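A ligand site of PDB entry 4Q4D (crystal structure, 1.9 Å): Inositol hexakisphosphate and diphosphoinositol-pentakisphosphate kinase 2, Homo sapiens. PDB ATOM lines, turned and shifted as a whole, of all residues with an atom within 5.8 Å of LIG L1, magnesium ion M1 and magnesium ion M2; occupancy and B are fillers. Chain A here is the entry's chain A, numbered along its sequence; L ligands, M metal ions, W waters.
The side-chain carboxylate (OD2) of Asp 273 binds magnesium ion M2. O1 of LIG L1 binds magnesium ion M2, 2.0 Å away. Magnesium ion M2 is bound by O7 of LIG L1 (2.1 Å). Water W6 is bound to magnesium ion M2 (2.1 Å). OD2 of Asp 285 binds magnesium ion M2.
The backbone NH (N) of Cys 284 is in hydrogen-bond range of the backbone carbonyl oxygen (O) of Asp 273 (3.1 Å). The side-chain amino group (NZ) of Lys 151 lies within salt-bridge range of the side-chain carboxylate (OE1) of Glu 201 (3.1 Å). The side-chain amino group of Lys 151 is in hydrogen-bond range of the backbone carbonyl oxygen of Cys 284 (2.9 Å). The side-chain hydroxyl (OH) of Tyr 102 is in hydrogen-bond range of the side-chain amino group (NZ) of Lys 151, 3.2 Å away. N of Glu 201 sits at hydrogen-bond distance from O of Val 149 (2.8 Å). The side-chain carboxylate (OE2) of Glu 201 lies within hydrogen-bond range of the side-chain hydroxyl (OH) of Tyr 102 (2.7 Å). The guanidinium group (NH2) of Arg 98 lies within hydrogen-bond range of the backbone carbonyl oxygen (O) of Asp 157, 2.8 Å away. The backbone carbonyl oxygen (O) of Cys 284 lies within hydrogen-bond range of the side-chain hydroxyl (OH) of Tyr 102, at 3.1 Å.
Water W2 bridges N6 of LIG L1 (2.9 Å) and OG of Ser 228 (3.4 Å). Water W5 bridges O of His 158 (2.7 Å) and O5 of LIG L1 (2.9 Å).
The side-chain carboxylate (OD1) of Asp 210 sits at hydrogen-bond distance from an oxygen (O12) of LIG L1, at 2.5 Å. ND1 of His 158 is in hydrogen-bond range of O5 of LIG L1, 2.7 Å away. NZ of Lys 151 lies within salt-bridge range of O6 of LIG L1 (2.7 Å). An oxygen (O12) of LIG L1 sits at hydrogen-bond distance from the side-chain hydroxyl (OG) of Ser 228, at 2.8 Å. A nitrogen (N5) of LIG L1 is in hydrogen-bond range of the backbone NH (N) of Met 204 (2.8 Å). OE1 of Glu 201 sits at hydrogen-bond distance from N4 of LIG L1, at 2.8 Å. A nitrogen (N4) of LIG L1 lies within hydrogen-bond range of the backbone carbonyl oxygen (O) of Glu 202 (2.8 Å). NH2 of Arg 98 lies within salt-bridge range of O5 of LIG L1 (3.2 Å). The side-chain amino group (NZ) of Lys 212 lies close to an oxygen (O1) of LIG L1 (3.5 Å). An oxygen (O19) of LG2 L2 is in salt-bridge range of the side-chain amino group of Lys 212, 3.6 Å away.
Magnesium ion M1 is bound by water W1, O3 of LIG L1, OD1 of Asn 287, O4 of LIG L1, OD2 of Asp 285 and OD1 of Asp 285.
Within 4 Å of magnesium ion M1: Asp 285 and Asn 287.
Within 4 Å of magnesium ion M2: Asp 273 and Asp 285.
The backbone carbonyl oxygen of Cys 284 lies close to an oxygen (O6) of LIG L1 (3.3 Å). Pro 113 touches LIG L1. CG2 of Val 149 touches C8 of LIG L1, at 3.7 Å. Val 160 touches LIG L1. CD2 of Leu 175 touches O10 of LIG L1 (3.4 Å). CD1 of Phe 203 touches C9 of LIG L1, 3.4 Å away. CD of Pro 229 touches O12 of LIG L1, 3.7 Å away. Leu 275 touches LIG L1 (CD1 to C8, 3.6 Å). Of the 29 residues printed, 20 come within 4 Å of LIG L1. Along chain A the residues within 4 Å of LIG L1 span positions 98 to 287.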
ATOM      1  N   ARG A  98      -5.793   3.057  -5.660  1.00  0.00           N
ATOM      2  CA  ARG A  98      -5.315   4.286  -6.314  1.00  0.00           C
ATOM      3  C   ARG A  98      -4.341   4.048  -7.468  1.00  0.00           C
ATOM      4  O   ARG A  98      -4.297   4.827  -8.426  1.00  0.00           O
ATOM      5  CB  ARG A  98      -4.649   5.209  -5.292  1.00  0.00           C
ATOM      6  CG  ARG A  98      -5.574   5.723  -4.220  1.00  0.00           C
ATOM      7  CD  ARG A  98      -4.842   6.785  -3.416  1.00  0.00           C
ATOM      8  NE  ARG A  98      -5.396   6.899  -2.086  1.00  0.00           N
ATOM      9  CZ  ARG A  98      -6.341   7.774  -1.722  1.00  0.00           C
ATOM     10  NH1 ARG A  98      -6.834   8.652  -2.606  1.00  0.00           N
ATOM     11  NH2 ARG A  98      -6.809   7.748  -0.490  1.00  0.00           N
ATOM     12  N   TYR A 102      -5.105   5.628 -11.162  1.00  0.00           N
ATOM     13  CA  TYR A 102      -4.138   6.482 -11.861  1.00  0.00           C
ATOM     14  C   TYR A 102      -3.701   5.843 -13.173  1.00  0.00           C
ATOM     15  O   TYR A 102      -3.545   6.531 -14.169  1.00  0.00           O
ATOM     16  CB  TYR A 102      -2.948   6.773 -10.934  1.00  0.00           C
ATOM     17  CG  TYR A 102      -3.132   7.982 -10.043  1.00  0.00           C
ATOM     18  CD1 TYR A 102      -4.389   8.346  -9.545  1.00  0.00           C
ATOM     19  CD2 TYR A 102      -2.044   8.767  -9.695  1.00  0.00           C
ATOM     20  CE1 TYR A 102      -4.548   9.484  -8.750  1.00  0.00           C
ATOM     21  CE2 TYR A 102      -2.181   9.923  -8.908  1.00  0.00           C
ATOM     22  CZ  TYR A 102      -3.422  10.280  -8.432  1.00  0.00           C
ATOM     23  OH  TYR A 102      -3.541  11.423  -7.646  1.00  0.00           O
ATOM     24  N   PRO A 113      -1.419  14.557 -11.474  1.00  0.00           N
ATOM     25  CA  PRO A 113      -0.107  14.919 -10.930  1.00  0.00           C
ATOM     26  C   PRO A 113       0.969  13.904 -11.306  1.00  0.00           C
ATOM     27  O   PRO A 113       0.694  12.700 -11.372  1.00  0.00           O
ATOM     28  CB  PRO A 113      -0.333  14.903  -9.415  1.00  0.00           C
ATOM     29  CG  PRO A 113      -1.800  15.033  -9.233  1.00  0.00           C
ATOM     30  CD  PRO A 113      -2.430  14.392 -10.428  1.00  0.00           C
ATOM     31  N   VAL A 149       2.926  14.950  -1.936  1.00  0.00           N
ATOM     32  CA  VAL A 149       1.779  14.305  -1.338  1.00  0.00           C
ATOM     33  C   VAL A 149       2.010  12.803  -1.289  1.00  0.00           C
ATOM     34  O   VAL A 149       2.519  12.204  -2.260  1.00  0.00           O
ATOM     35  CB  VAL A 149       0.523  14.640  -2.183  1.00  0.00           C
ATOM     36  CG1 VAL A 149      -0.721  14.037  -1.593  1.00  0.00           C
ATOM     37  CG2 VAL A 149       0.401  16.154  -2.326  1.00  0.00           C
ATOM     38  N   LYS A 151      -0.045   9.275  -0.509  1.00  0.00           N
ATOM     39  CA  LYS A 151      -1.381   8.678  -0.417  1.00  0.00           C
ATOM     40  C   LYS A 151      -1.284   7.145  -0.225  1.00  0.00           C
ATOM     41  O   LYS A 151      -0.585   6.480  -0.975  1.00  0.00           O
ATOM     42  CB  LYS A 151      -2.169   8.965  -1.681  1.00  0.00           C
ATOM     43  CG  LYS A 151      -2.324  10.425  -2.036  1.00  0.00           C
ATOM     44  CD  LYS A 151      -3.297  10.599  -3.197  1.00  0.00           C
ATOM     45  CE  LYS A 151      -3.392  12.069  -3.575  1.00  0.00           C
ATOM     46  NZ  LYS A 151      -4.306  12.332  -4.710  1.00  0.00           N
ATOM     47  N   ALA A 155      -7.605   3.313  -1.813  1.00  0.00           N
ATOM     48  CA  ALA A 155      -8.394   4.532  -2.004  1.00  0.00           C
ATOM     49  C   ALA A 155      -9.390   4.708  -0.868  1.00  0.00           C
ATOM     50  O   ALA A 155      -9.942   5.791  -0.671  1.00  0.00           O
ATOM     51  CB  ALA A 155      -9.134   4.464  -3.336  1.00  0.00           C
ATOM     52  N   ASP A 157      -8.505   4.369   2.226  1.00  0.00           N
ATOM     53  CA  ASP A 157      -7.736   4.910   3.359  1.00  0.00           C
ATOM     54  C   ASP A 157      -7.471   6.379   3.058  1.00  0.00           C
ATOM     55  O   ASP A 157      -6.692   6.706   2.133  1.00  0.00           O
ATOM     56  CB  ASP A 157      -6.446   4.089   3.550  1.00  0.00           C
ATOM     57  CG  ASP A 157      -5.569   4.580   4.701  1.00  0.00           C
ATOM     58  OD1 ASP A 157      -5.763   5.707   5.226  1.00  0.00           O
ATOM     59  OD2 ASP A 157      -4.610   3.855   5.033  1.00  0.00           O
ATOM     60  N   HIS A 158      -8.137   7.256   3.811  1.00  0.00           N
ATOM     61  CA  HIS A 158      -8.076   8.721   3.579  1.00  0.00           C
ATOM     62  C   HIS A 158      -6.975   9.476   4.351  1.00  0.00           C
ATOM     63  O   HIS A 158      -6.986  10.703   4.405  1.00  0.00           O
ATOM     64  CB  HIS A 158      -9.457   9.300   3.873  1.00  0.00           C
ATOM     65  CG  HIS A 158     -10.539   8.622   3.087  1.00  0.00           C
ATOM     66  ND1 HIS A 158     -10.567   8.633   1.712  1.00  0.00           N
ATOM     67  CD2 HIS A 158     -11.570   7.832   3.459  1.00  0.00           C
ATOM     68  CE1 HIS A 158     -11.586   7.916   1.280  1.00  0.00           C
ATOM     69  NE2 HIS A 158     -12.218   7.419   2.326  1.00  0.00           N
ATOM     70  N   ASN A 159      -6.056   8.733   4.960  1.00  0.00           N
ATOM     71  CA  ASN A 159      -4.888   9.262   5.660  1.00  0.00           C
ATOM     72  C   ASN A 159      -3.785   9.701   4.668  1.00  0.00           C
ATOM     73  O   ASN A 159      -2.722   9.114   4.569  1.00  0.00           O
ATOM     74  CB  ASN A 159      -4.402   8.246   6.689  1.00  0.00           C
ATOM     75  CG  ASN A 159      -5.459   7.967   7.750  1.00  0.00           C
ATOM     76  OD1 ASN A 159      -5.762   8.836   8.540  1.00  0.00           O
ATOM     77  ND2 ASN A 159      -6.053   6.769   7.732  1.00  0.00           N
ATOM     78  N   VAL A 160      -4.101  10.761   3.951  1.00  0.00           N
ATOM     79  CA  VAL A 160      -3.204  11.372   2.982  1.00  0.00           C
ATOM     80  C   VAL A 160      -2.363  12.417   3.707  1.00  0.00           C
ATOM     81  O   VAL A 160      -2.904  13.265   4.442  1.00  0.00           O
ATOM     82  CB  VAL A 160      -4.025  12.018   1.876  1.00  0.00           C
ATOM     83  CG1 VAL A 160      -3.192  12.900   0.951  1.00  0.00           C
ATOM     84  CG2 VAL A 160      -4.728  10.934   1.081  1.00  0.00           C
ATOM     85  N   ILE A 162       0.748  15.491   3.478  1.00  0.00           N
ATOM     86  CA  ILE A 162       1.465  16.500   2.668  1.00  0.00           C
ATOM     87  C   ILE A 162       2.707  16.891   3.447  1.00  0.00           C
ATOM     88  O   ILE A 162       2.619  17.181   4.644  1.00  0.00           O
ATOM     89  CB  ILE A 162       0.632  17.783   2.466  1.00  0.00           C
ATOM     90  CG1 ILE A 162      -0.812  17.490   2.049  1.00  0.00           C
ATOM     91  CG2 ILE A 162       1.329  18.722   1.475  1.00  0.00           C
ATOM     92  CD1 ILE A 162      -1.024  16.546   0.935  1.00  0.00           C
ATOM     93  N   LEU A 175      -4.085  14.562   6.667  1.00  0.00           N
ATOM     94  CA  LEU A 175      -5.512  14.603   6.300  1.00  0.00           C
ATOM     95  C   LEU A 175      -6.202  13.336   6.762  1.00  0.00           C
ATOM     96  O   LEU A 175      -5.568  12.310   6.953  1.00  0.00           O
ATOM     97  CB  LEU A 175      -5.705  14.753   4.791  1.00  0.00           C
ATOM     98  CG  LEU A 175      -5.372  16.085   4.159  1.00  0.00           C
ATOM     99  CD1 LEU A 175      -3.941  16.536   4.410  1.00  0.00           C
ATOM    100  CD2 LEU A 175      -5.684  16.048   2.659  1.00  0.00           C
ATOM    101  N   GLU A 201       3.213  11.890  -4.995  1.00  0.00           N
ATOM    102  CA  GLU A 201       2.940  12.747  -6.142  1.00  0.00           C
ATOM    103  C   GLU A 201       3.261  14.202  -5.897  1.00  0.00           C
ATOM    104  O   GLU A 201       3.309  14.692  -4.745  1.00  0.00           O
ATOM    105  CB  GLU A 201       1.505  12.585  -6.622  1.00  0.00           C
ATOM    106  CG  GLU A 201       0.460  12.847  -5.613  1.00  0.00           C
ATOM    107  CD  GLU A 201      -0.946  12.495  -6.049  1.00  0.00           C
ATOM    108  OE1 GLU A 201      -1.756  13.424  -6.099  1.00  0.00           O
ATOM    109  OE2 GLU A 201      -1.298  11.319  -6.238  1.00  0.00           O
ATOM    110  N   GLU A 202       3.458  14.919  -6.987  1.00  0.00           N
ATOM    111  CA  GLU A 202       3.774  16.323  -6.918  1.00  0.00           C
ATOM    112  C   GLU A 202       2.577  17.124  -6.394  1.00  0.00           C
ATOM    113  O   GLU A 202       1.417  16.790  -6.662  1.00  0.00           O
ATOM    114  CB  GLU A 202       4.270  16.804  -8.275  1.00  0.00           C
ATOM    115  CG  GLU A 202       3.556  17.998  -8.857  1.00  0.00           C
ATOM    116  CD  GLU A 202       4.192  18.443 -10.142  1.00  0.00           C
ATOM    117  OE1 GLU A 202       3.489  19.155 -10.900  1.00  0.00           O
ATOM    118  OE2 GLU A 202       5.358  18.048 -10.413  1.00  0.00           O
ATOM    119  N   PHE A 203       2.872  18.128  -5.582  1.00  0.00           N
ATOM    120  CA  PHE A 203       1.846  18.996  -5.017  1.00  0.00           C
ATOM    121  C   PHE A 203       1.453  20.038  -6.067  1.00  0.00           C
ATOM    122  O   PHE A 203       2.305  20.797  -6.566  1.00  0.00           O
ATOM    123  CB  PHE A 203       2.364  19.712  -3.761  1.00  0.00           C
ATOM    124  CG  PHE A 203       1.353  20.610  -3.132  1.00  0.00           C
ATOM    125  CD1 PHE A 203       0.401  20.097  -2.281  1.00  0.00           C
ATOM    126  CD2 PHE A 203       1.362  21.973  -3.400  1.00  0.00           C
ATOM    127  CE1 PHE A 203      -0.546  20.929  -1.695  1.00  0.00           C
ATOM    128  CE2 PHE A 203       0.418  22.824  -2.818  1.00  0.00           C
ATOM    129  CZ  PHE A 203      -0.540  22.281  -1.971  1.00  0.00           C
ATOM    130  N   MET A 204       0.167  20.071  -6.377  1.00  0.00           N
ATOM    131  CA  MET A 204      -0.385  21.010  -7.362  1.00  0.00           C
ATOM    132  C   MET A 204      -0.922  22.234  -6.644  1.00  0.00           C
ATOM    133  O   MET A 204      -1.889  22.127  -5.882  1.00  0.00           O
ATOM    134  CB  MET A 204      -1.497  20.362  -8.178  1.00  0.00           C
ATOM    135  CG  MET A 204      -1.174  18.978  -8.740  1.00  0.00           C
ATOM    136  SD  MET A 204       0.315  18.848  -9.728  1.00  0.00           S
ATOM    137  CE  MET A 204      -0.011  19.974 -11.070  1.00  0.00           C
ATOM    138  N   PRO A 205      -0.338  23.412  -6.919  1.00  0.00           N
ATOM    139  CA  PRO A 205      -0.784  24.616  -6.246  1.00  0.00           C
ATOM    140  C   PRO A 205      -2.122  25.104  -6.800  1.00  0.00           C
ATOM    141  O   PRO A 205      -2.228  25.351  -7.990  1.00  0.00           O
ATOM    142  CB  PRO A 205       0.292  25.618  -6.608  1.00  0.00           C
ATOM    143  CG  PRO A 205       0.736  25.197  -7.953  1.00  0.00           C
ATOM    144  CD  PRO A 205       0.699  23.703  -7.928  1.00  0.00           C
ATOM    145  N   THR A 206      -3.121  25.240  -5.956  1.00  0.00           N
ATOM    146  CA  THR A 206      -4.454  25.698  -6.383  1.00  0.00           C
ATOM    147  C   THR A 206      -4.718  26.987  -5.623  1.00  0.00           C
ATOM    148  O   THR A 206      -3.864  27.429  -4.882  1.00  0.00           O
ATOM    149  CB  THR A 206      -5.543  24.696  -5.978  1.00  0.00           C
ATOM    150  OG1 THR A 206      -5.610  24.595  -4.542  1.00  0.00           O
ATOM    151  CG2 THR A 206      -5.291  23.345  -6.573  1.00  0.00           C
ATOM    152  N   ASP A 210     -10.706  22.709  -3.761  1.00  0.00           N
ATOM    153  CA  ASP A 210     -10.785  21.505  -4.573  1.00  0.00           C
ATOM    154  C   ASP A 210     -12.060  21.612  -5.390  1.00  0.00           C
ATOM    155  O   ASP A 210     -13.055  22.104  -4.847  1.00  0.00           O
ATOM    156  CB  ASP A 210     -11.005  20.252  -3.696  1.00  0.00           C
ATOM    157  CG  ASP A 210      -9.873  19.966  -2.774  1.00  0.00           C
ATOM    158  OD1 ASP A 210      -8.718  20.317  -3.114  1.00  0.00           O
ATOM    159  OD2 ASP A 210     -10.184  19.304  -1.742  1.00  0.00           O
ATOM    160  N   LYS A 212     -15.040  19.485  -6.860  1.00  0.00           N
ATOM    161  CA  LYS A 212     -15.672  18.170  -6.812  1.00  0.00           C
ATOM    162  C   LYS A 212     -16.667  18.043  -7.954  1.00  0.00           C
ATOM    163  O   LYS A 212     -17.516  18.924  -8.134  1.00  0.00           O
ATOM    164  CB  LYS A 212     -16.394  17.997  -5.489  1.00  0.00           C
ATOM    165  CG  LYS A 212     -15.534  18.386  -4.289  1.00  0.00           C
ATOM    166  CD  LYS A 212     -14.797  17.246  -3.679  1.00  0.00           C
ATOM    167  CE  LYS A 212     -15.688  16.219  -2.978  1.00  0.00           C
ATOM    168  NZ  LYS A 212     -14.878  14.971  -2.818  1.00  0.00           N
ATOM    169  N   SER A 228      -9.781  23.351   0.484  1.00  0.00           N
ATOM    170  CA  SER A 228      -8.921  22.167   0.512  1.00  0.00           C
ATOM    171  C   SER A 228      -8.621  21.768   1.966  1.00  0.00           C
ATOM    172  O   SER A 228      -8.194  22.614   2.726  1.00  0.00           O
ATOM    173  CB  SER A 228      -7.576  22.411  -0.135  1.00  0.00           C
ATOM    174  OG  SER A 228      -6.816  21.222   0.036  1.00  0.00           O
ATOM    175  N   PRO A 229      -8.787  20.481   2.324  1.00  0.00           N
ATOM    176  CA  PRO A 229      -8.405  20.046   3.686  1.00  0.00           C
ATOM    177  C   PRO A 229      -6.922  20.243   3.987  1.00  0.00           C
ATOM    178  O   PRO A 229      -6.548  20.440   5.152  1.00  0.00           O
ATOM    179  CB  PRO A 229      -8.760  18.542   3.721  1.00  0.00           C
ATOM    180  CG  PRO A 229      -9.408  18.216   2.441  1.00  0.00           C
ATOM    181  CD  PRO A 229      -9.295  19.377   1.495  1.00  0.00           C
ATOM    182  N   ALA A 230      -6.103  20.217   2.943  1.00  0.00           N
ATOM    183  CA  ALA A 230      -4.680  20.492   3.059  1.00  0.00           C
ATOM    184  C   ALA A 230      -4.317  21.927   3.515  1.00  0.00           C
ATOM    185  O   ALA A 230      -3.139  22.202   3.697  1.00  0.00           O
ATOM    186  CB  ALA A 230      -4.012  20.189   1.725  1.00  0.00           C
ATOM    187  N   ASP A 273     -12.379  14.300  -8.283  1.00  0.00           N
ATOM    188  CA  ASP A 273     -11.860  15.587  -7.802  1.00  0.00           C
ATOM    189  C   ASP A 273     -10.873  16.160  -8.812  1.00  0.00           C
ATOM    190  O   ASP A 273     -10.062  15.413  -9.365  1.00  0.00           O
ATOM    191  CB  ASP A 273     -11.144  15.415  -6.459  1.00  0.00           C
ATOM    192  CG  ASP A 273     -12.082  14.934  -5.359  1.00  0.00           C
ATOM    193  OD1 ASP A 273     -13.269  15.346  -5.354  1.00  0.00           O
ATOM    194  OD2 ASP A 273     -11.619  14.201  -4.482  1.00  0.00           O
ATOM    195  N   LEU A 275      -8.054  19.461  -9.474  1.00  0.00           N
ATOM    196  CA  LEU A 275      -7.220  20.482  -8.950  1.00  0.00           C
ATOM    197  C   LEU A 275      -6.947  21.452 -10.062  1.00  0.00           C
ATOM    198  O   LEU A 275      -6.342  21.077 -11.085  1.00  0.00           O
ATOM    199  CB  LEU A 275      -5.896  19.903  -8.462  1.00  0.00           C
ATOM    200  CG  LEU A 275      -5.996  18.796  -7.423  1.00  0.00           C
ATOM    201  CD1 LEU A 275      -4.606  18.248  -7.127  1.00  0.00           C
ATOM    202  CD2 LEU A 275      -6.730  19.235  -6.180  1.00  0.00           C
ATOM    203  N   CYS A 284      -7.246  14.179  -9.293  1.00  0.00           N
ATOM    204  CA  CYS A 284      -6.439  13.602  -8.215  1.00  0.00           C
ATOM    205  C   CYS A 284      -7.066  12.440  -7.461  1.00  0.00           C
ATOM    206  O   CYS A 284      -6.407  11.829  -6.628  1.00  0.00           O
ATOM    207  CB  CYS A 284      -5.963  14.675  -7.231  1.00  0.00           C
ATOM    208  SG  CYS A 284      -7.246  15.316  -6.153  1.00  0.00           S
ATOM    209  N   ASP A 285      -8.303  12.091  -7.815  1.00  0.00           N
ATOM    210  CA  ASP A 285      -9.059  11.114  -7.086  1.00  0.00           C
ATOM    211  C   ASP A 285     -10.305  10.826  -7.921  1.00  0.00           C
ATOM    212  O   ASP A 285     -10.933  11.756  -8.427  1.00  0.00           O
ATOM    213  CB  ASP A 285      -9.443  11.714  -5.726  1.00  0.00           C
ATOM    214  CG  ASP A 285     -10.112  10.742  -4.787  1.00  0.00           C
ATOM    215  OD1 ASP A 285      -9.857   9.541  -4.870  1.00  0.00           O
ATOM    216  OD2 ASP A 285     -10.869  11.197  -3.882  1.00  0.00           O
ATOM    217  N   VAL A 286     -10.648   9.552  -8.025  1.00  0.00           N
ATOM    218  CA  VAL A 286     -11.925   9.136  -8.619  1.00  0.00           C
ATOM    219  C   VAL A 286     -12.618   8.245  -7.585  1.00  0.00           C
ATOM    220  O   VAL A 286     -12.069   7.218  -7.163  1.00  0.00           O
ATOM    221  CB  VAL A 286     -11.695   8.322  -9.907  1.00  0.00           C
ATOM    222  CG1 VAL A 286     -13.013   7.813 -10.480  1.00  0.00           C
ATOM    223  CG2 VAL A 286     -10.948   9.157 -10.933  1.00  0.00           C
ATOM    224  N   ASN A 287     -13.810   8.648  -7.166  1.00  0.00           N
ATOM    225  CA  ASN A 287     -14.527   8.006  -6.072  1.00  0.00           C
ATOM    226  C   ASN A 287     -15.647   7.062  -6.472  1.00  0.00           C
ATOM    227  O   ASN A 287     -16.105   6.259  -5.649  1.00  0.00           O
ATOM    228  CB  ASN A 287     -15.040   9.072  -5.119  1.00  0.00           C
ATOM    229  CG  ASN A 287     -13.909   9.769  -4.427  1.00  0.00           C
ATOM    230  OD1 ASN A 287     -12.931   9.113  -4.038  1.00  0.00           O
ATOM    231  ND2 ASN A 287     -14.005  11.074  -4.276  1.00  0.00           N
HETATM  232  P1  LIG L   1     -12.151  11.501  -0.851  1.00  0.00           P
HETATM  233  O1  LIG L   1     -12.452  12.559  -1.920  1.00  0.00           O
HETATM  234  O2  LIG L   1     -12.820  11.813   0.471  1.00  0.00           O
HETATM  235  O3  LIG L   1     -12.202  10.054  -1.333  1.00  0.00           O
HETATM  236  P2  LIG L   1      -9.159  10.873  -0.645  1.00  0.00           P
HETATM  237  O4  LIG L   1      -9.431   9.954  -1.834  1.00  0.00           O
HETATM  238  O5  LIG L   1      -8.658  10.118   0.547  1.00  0.00           O
HETATM  239  N1  LIG L   1     -10.505  11.921  -0.449  1.00  0.00           N
HETATM  240  P3  LIG L   1      -7.574  12.756  -2.283  1.00  0.00           P
HETATM  241  O6  LIG L   1      -6.679  12.175  -3.349  1.00  0.00           O
HETATM  242  O7  LIG L   1      -8.869  13.376  -2.690  1.00  0.00           O
HETATM  243  O8  LIG L   1      -7.810  11.708  -1.063  1.00  0.00           O
HETATM  244  O9  LIG L   1      -6.720  13.839  -1.443  1.00  0.00           O
HETATM  245  C1  LIG L   1      -7.381  14.642  -0.463  1.00  0.00           C
HETATM  246  C2  LIG L   1      -7.148  16.131  -0.731  1.00  0.00           C
HETATM  247  O10 LIG L   1      -5.754  16.409  -0.734  1.00  0.00           O
HETATM  248  C3  LIG L   1      -7.641  16.624  -2.070  1.00  0.00           C
HETATM  249  O11 LIG L   1      -9.039  16.921  -1.998  1.00  0.00           O
HETATM  250  C4  LIG L   1      -6.768  17.836  -2.302  1.00  0.00           C
HETATM  251  O12 LIG L   1      -7.213  19.006  -1.593  1.00  0.00           O
HETATM  252  C5  LIG L   1      -5.453  17.402  -1.690  1.00  0.00           C
HETATM  253  N2  LIG L   1      -4.571  16.794  -2.688  1.00  0.00           N
HETATM  254  C6  LIG L   1      -4.533  15.514  -3.089  1.00  0.00           C
HETATM  255  N3  LIG L   1      -3.590  15.325  -4.038  1.00  0.00           N
HETATM  256  C7  LIG L   1      -2.990  16.525  -4.238  1.00  0.00           C
HETATM  257  C8  LIG L   1      -1.906  17.031  -5.092  1.00  0.00           C
HETATM  258  N4  LIG L   1      -1.266  16.196  -5.919  1.00  0.00           N
HETATM  259  N5  LIG L   1      -1.570  18.345  -5.003  1.00  0.00           N
HETATM  260  C9  LIG L   1      -2.231  19.173  -4.171  1.00  0.00           C
HETATM  261  N6  LIG L   1      -3.235  18.763  -3.357  1.00  0.00           N
HETATM  262  C10 LIG L   1      -3.643  17.476  -3.344  1.00  0.00           C
HETATM  263  O1  LG2 L   2     -21.509  13.942   8.012  1.00  0.00           O
HETATM  264  P1  LG2 L   2     -20.701  15.091   7.195  1.00  0.00           P
HETATM  265  O2  LG2 L   2     -21.688  16.095   6.744  1.00  0.00           O
HETATM  266  O3  LG2 L   2     -19.480  15.528   7.930  1.00  0.00           O
HETATM  267  O4  LG2 L   2     -20.198  14.271   5.888  1.00  0.00           O
HETATM  268  P2  LG2 L   2     -19.262  12.914   5.917  1.00  0.00           P
HETATM  269  O5  LG2 L   2     -19.607  12.075   7.085  1.00  0.00           O
HETATM  270  O6  LG2 L   2     -17.854  13.289   5.660  1.00  0.00           O
HETATM  271  O7  LG2 L   2     -19.887  12.179   4.592  1.00  0.00           O
HETATM  272  C1  LG2 L   2     -19.078  11.798   3.501  1.00  0.00           C
HETATM  273  C2  LG2 L   2     -19.185  10.312   3.405  1.00  0.00           C
HETATM  274  O8  LG2 L   2     -18.617   9.769   4.625  1.00  0.00           O
HETATM  275  P3  LG2 L   2     -19.437   8.772   5.606  1.00  0.00           P
HETATM  276  O9  LG2 L   2     -20.859   9.057   5.417  1.00  0.00           O
HETATM  277  O10 LG2 L   2     -18.941   7.484   5.132  1.00  0.00           O
HETATM  278  O11 LG2 L   2     -18.909   9.211   6.922  1.00  0.00           O
HETATM  279  C3  LG2 L   2     -19.590  12.491   2.237  1.00  0.00           C
HETATM  280  O12 LG2 L   2     -19.322  13.895   2.388  1.00  0.00           O
HETATM  281  P4  LG2 L   2     -20.508  14.948   2.492  1.00  0.00           P
HETATM  282  O13 LG2 L   2     -21.731  14.189   2.792  1.00  0.00           O
HETATM  283  O14 LG2 L   2     -20.081  15.886   3.546  1.00  0.00           O
HETATM  284  O15 LG2 L   2     -20.439  15.494   1.091  1.00  0.00           O
HETATM  285  C4  LG2 L   2     -18.838  12.003   1.019  1.00  0.00           C
HETATM  286  O16 LG2 L   2     -19.476  12.609  -0.187  1.00  0.00           O
HETATM  287  P5  LG2 L   2     -18.633  13.704  -1.054  1.00  0.00           P
HETATM  288  O17 LG2 L   2     -19.553  14.079  -2.142  1.00  0.00           O
HETATM  289  O18 LG2 L   2     -18.331  14.768  -0.067  1.00  0.00           O
HETATM  290  O19 LG2 L   2     -17.460  12.887  -1.458  1.00  0.00           O
HETATM  291  C5  LG2 L   2     -18.881  10.460   0.930  1.00  0.00           C
HETATM  292  O20 LG2 L   2     -20.216  10.091   0.689  1.00  0.00           O
HETATM  293  P6  LG2 L   2     -20.681   9.459  -0.754  1.00  0.00           P
HETATM  294  O21 LG2 L   2     -22.095   9.840  -0.794  1.00  0.00           O
HETATM  295  O22 LG2 L   2     -19.842  10.052  -1.811  1.00  0.00           O
HETATM  296  O23 LG2 L   2     -20.392   8.019  -0.478  1.00  0.00           O
HETATM  297  C6  LG2 L   2     -18.384   9.828   2.238  1.00  0.00           C
HETATM  298  O24 LG2 L   2     -18.466   8.388   2.192  1.00  0.00           O
HETATM  299  P7  LG2 L   2     -17.239   7.574   1.490  1.00  0.00           P
HETATM  300  O25 LG2 L   2     -15.872   8.428   1.662  1.00  0.00           O
HETATM  301  O26 LG2 L   2     -17.530   7.358   0.034  1.00  0.00           O
HETATM  302  O27 LG2 L   2     -17.056   6.300   2.408  1.00  0.00           O
HETATM  303  P8  LG2 L   2     -18.175   5.138   2.401  1.00  0.00           P
HETATM  304  O28 LG2 L   2     -17.406   3.884   2.436  1.00  0.00           O
HETATM  305  O29 LG2 L   2     -19.001   5.400   3.564  1.00  0.00           O
HETATM  306  O30 LG2 L   2     -18.810   5.408   1.090  1.00  0.00           O
HETATM  307 MG    MG M   1     -11.201   9.327  -2.870  1.00  0.00          MG
HETATM  308 MG    MG M   2     -10.935  13.260  -2.935  1.00  0.00          MG
HETATM  309  O   HOH W   1     -11.053   7.613  -2.568  1.00  0.00           O
HETATM  310  O   HOH W   2      -4.401  21.243  -2.320  1.00  0.00           O
HETATM  311  O   HOH W   3     -14.606   8.692  -0.989  1.00  0.00           O
HETATM  312  O   HOH W   4     -11.295  12.452   3.063  1.00  0.00           O
HETATM  313  O   HOH W   5      -7.774  12.271   2.331  1.00  0.00           O
HETATM  314  O   HOH W   6     -10.966  15.137  -1.916  1.00  0.00           O
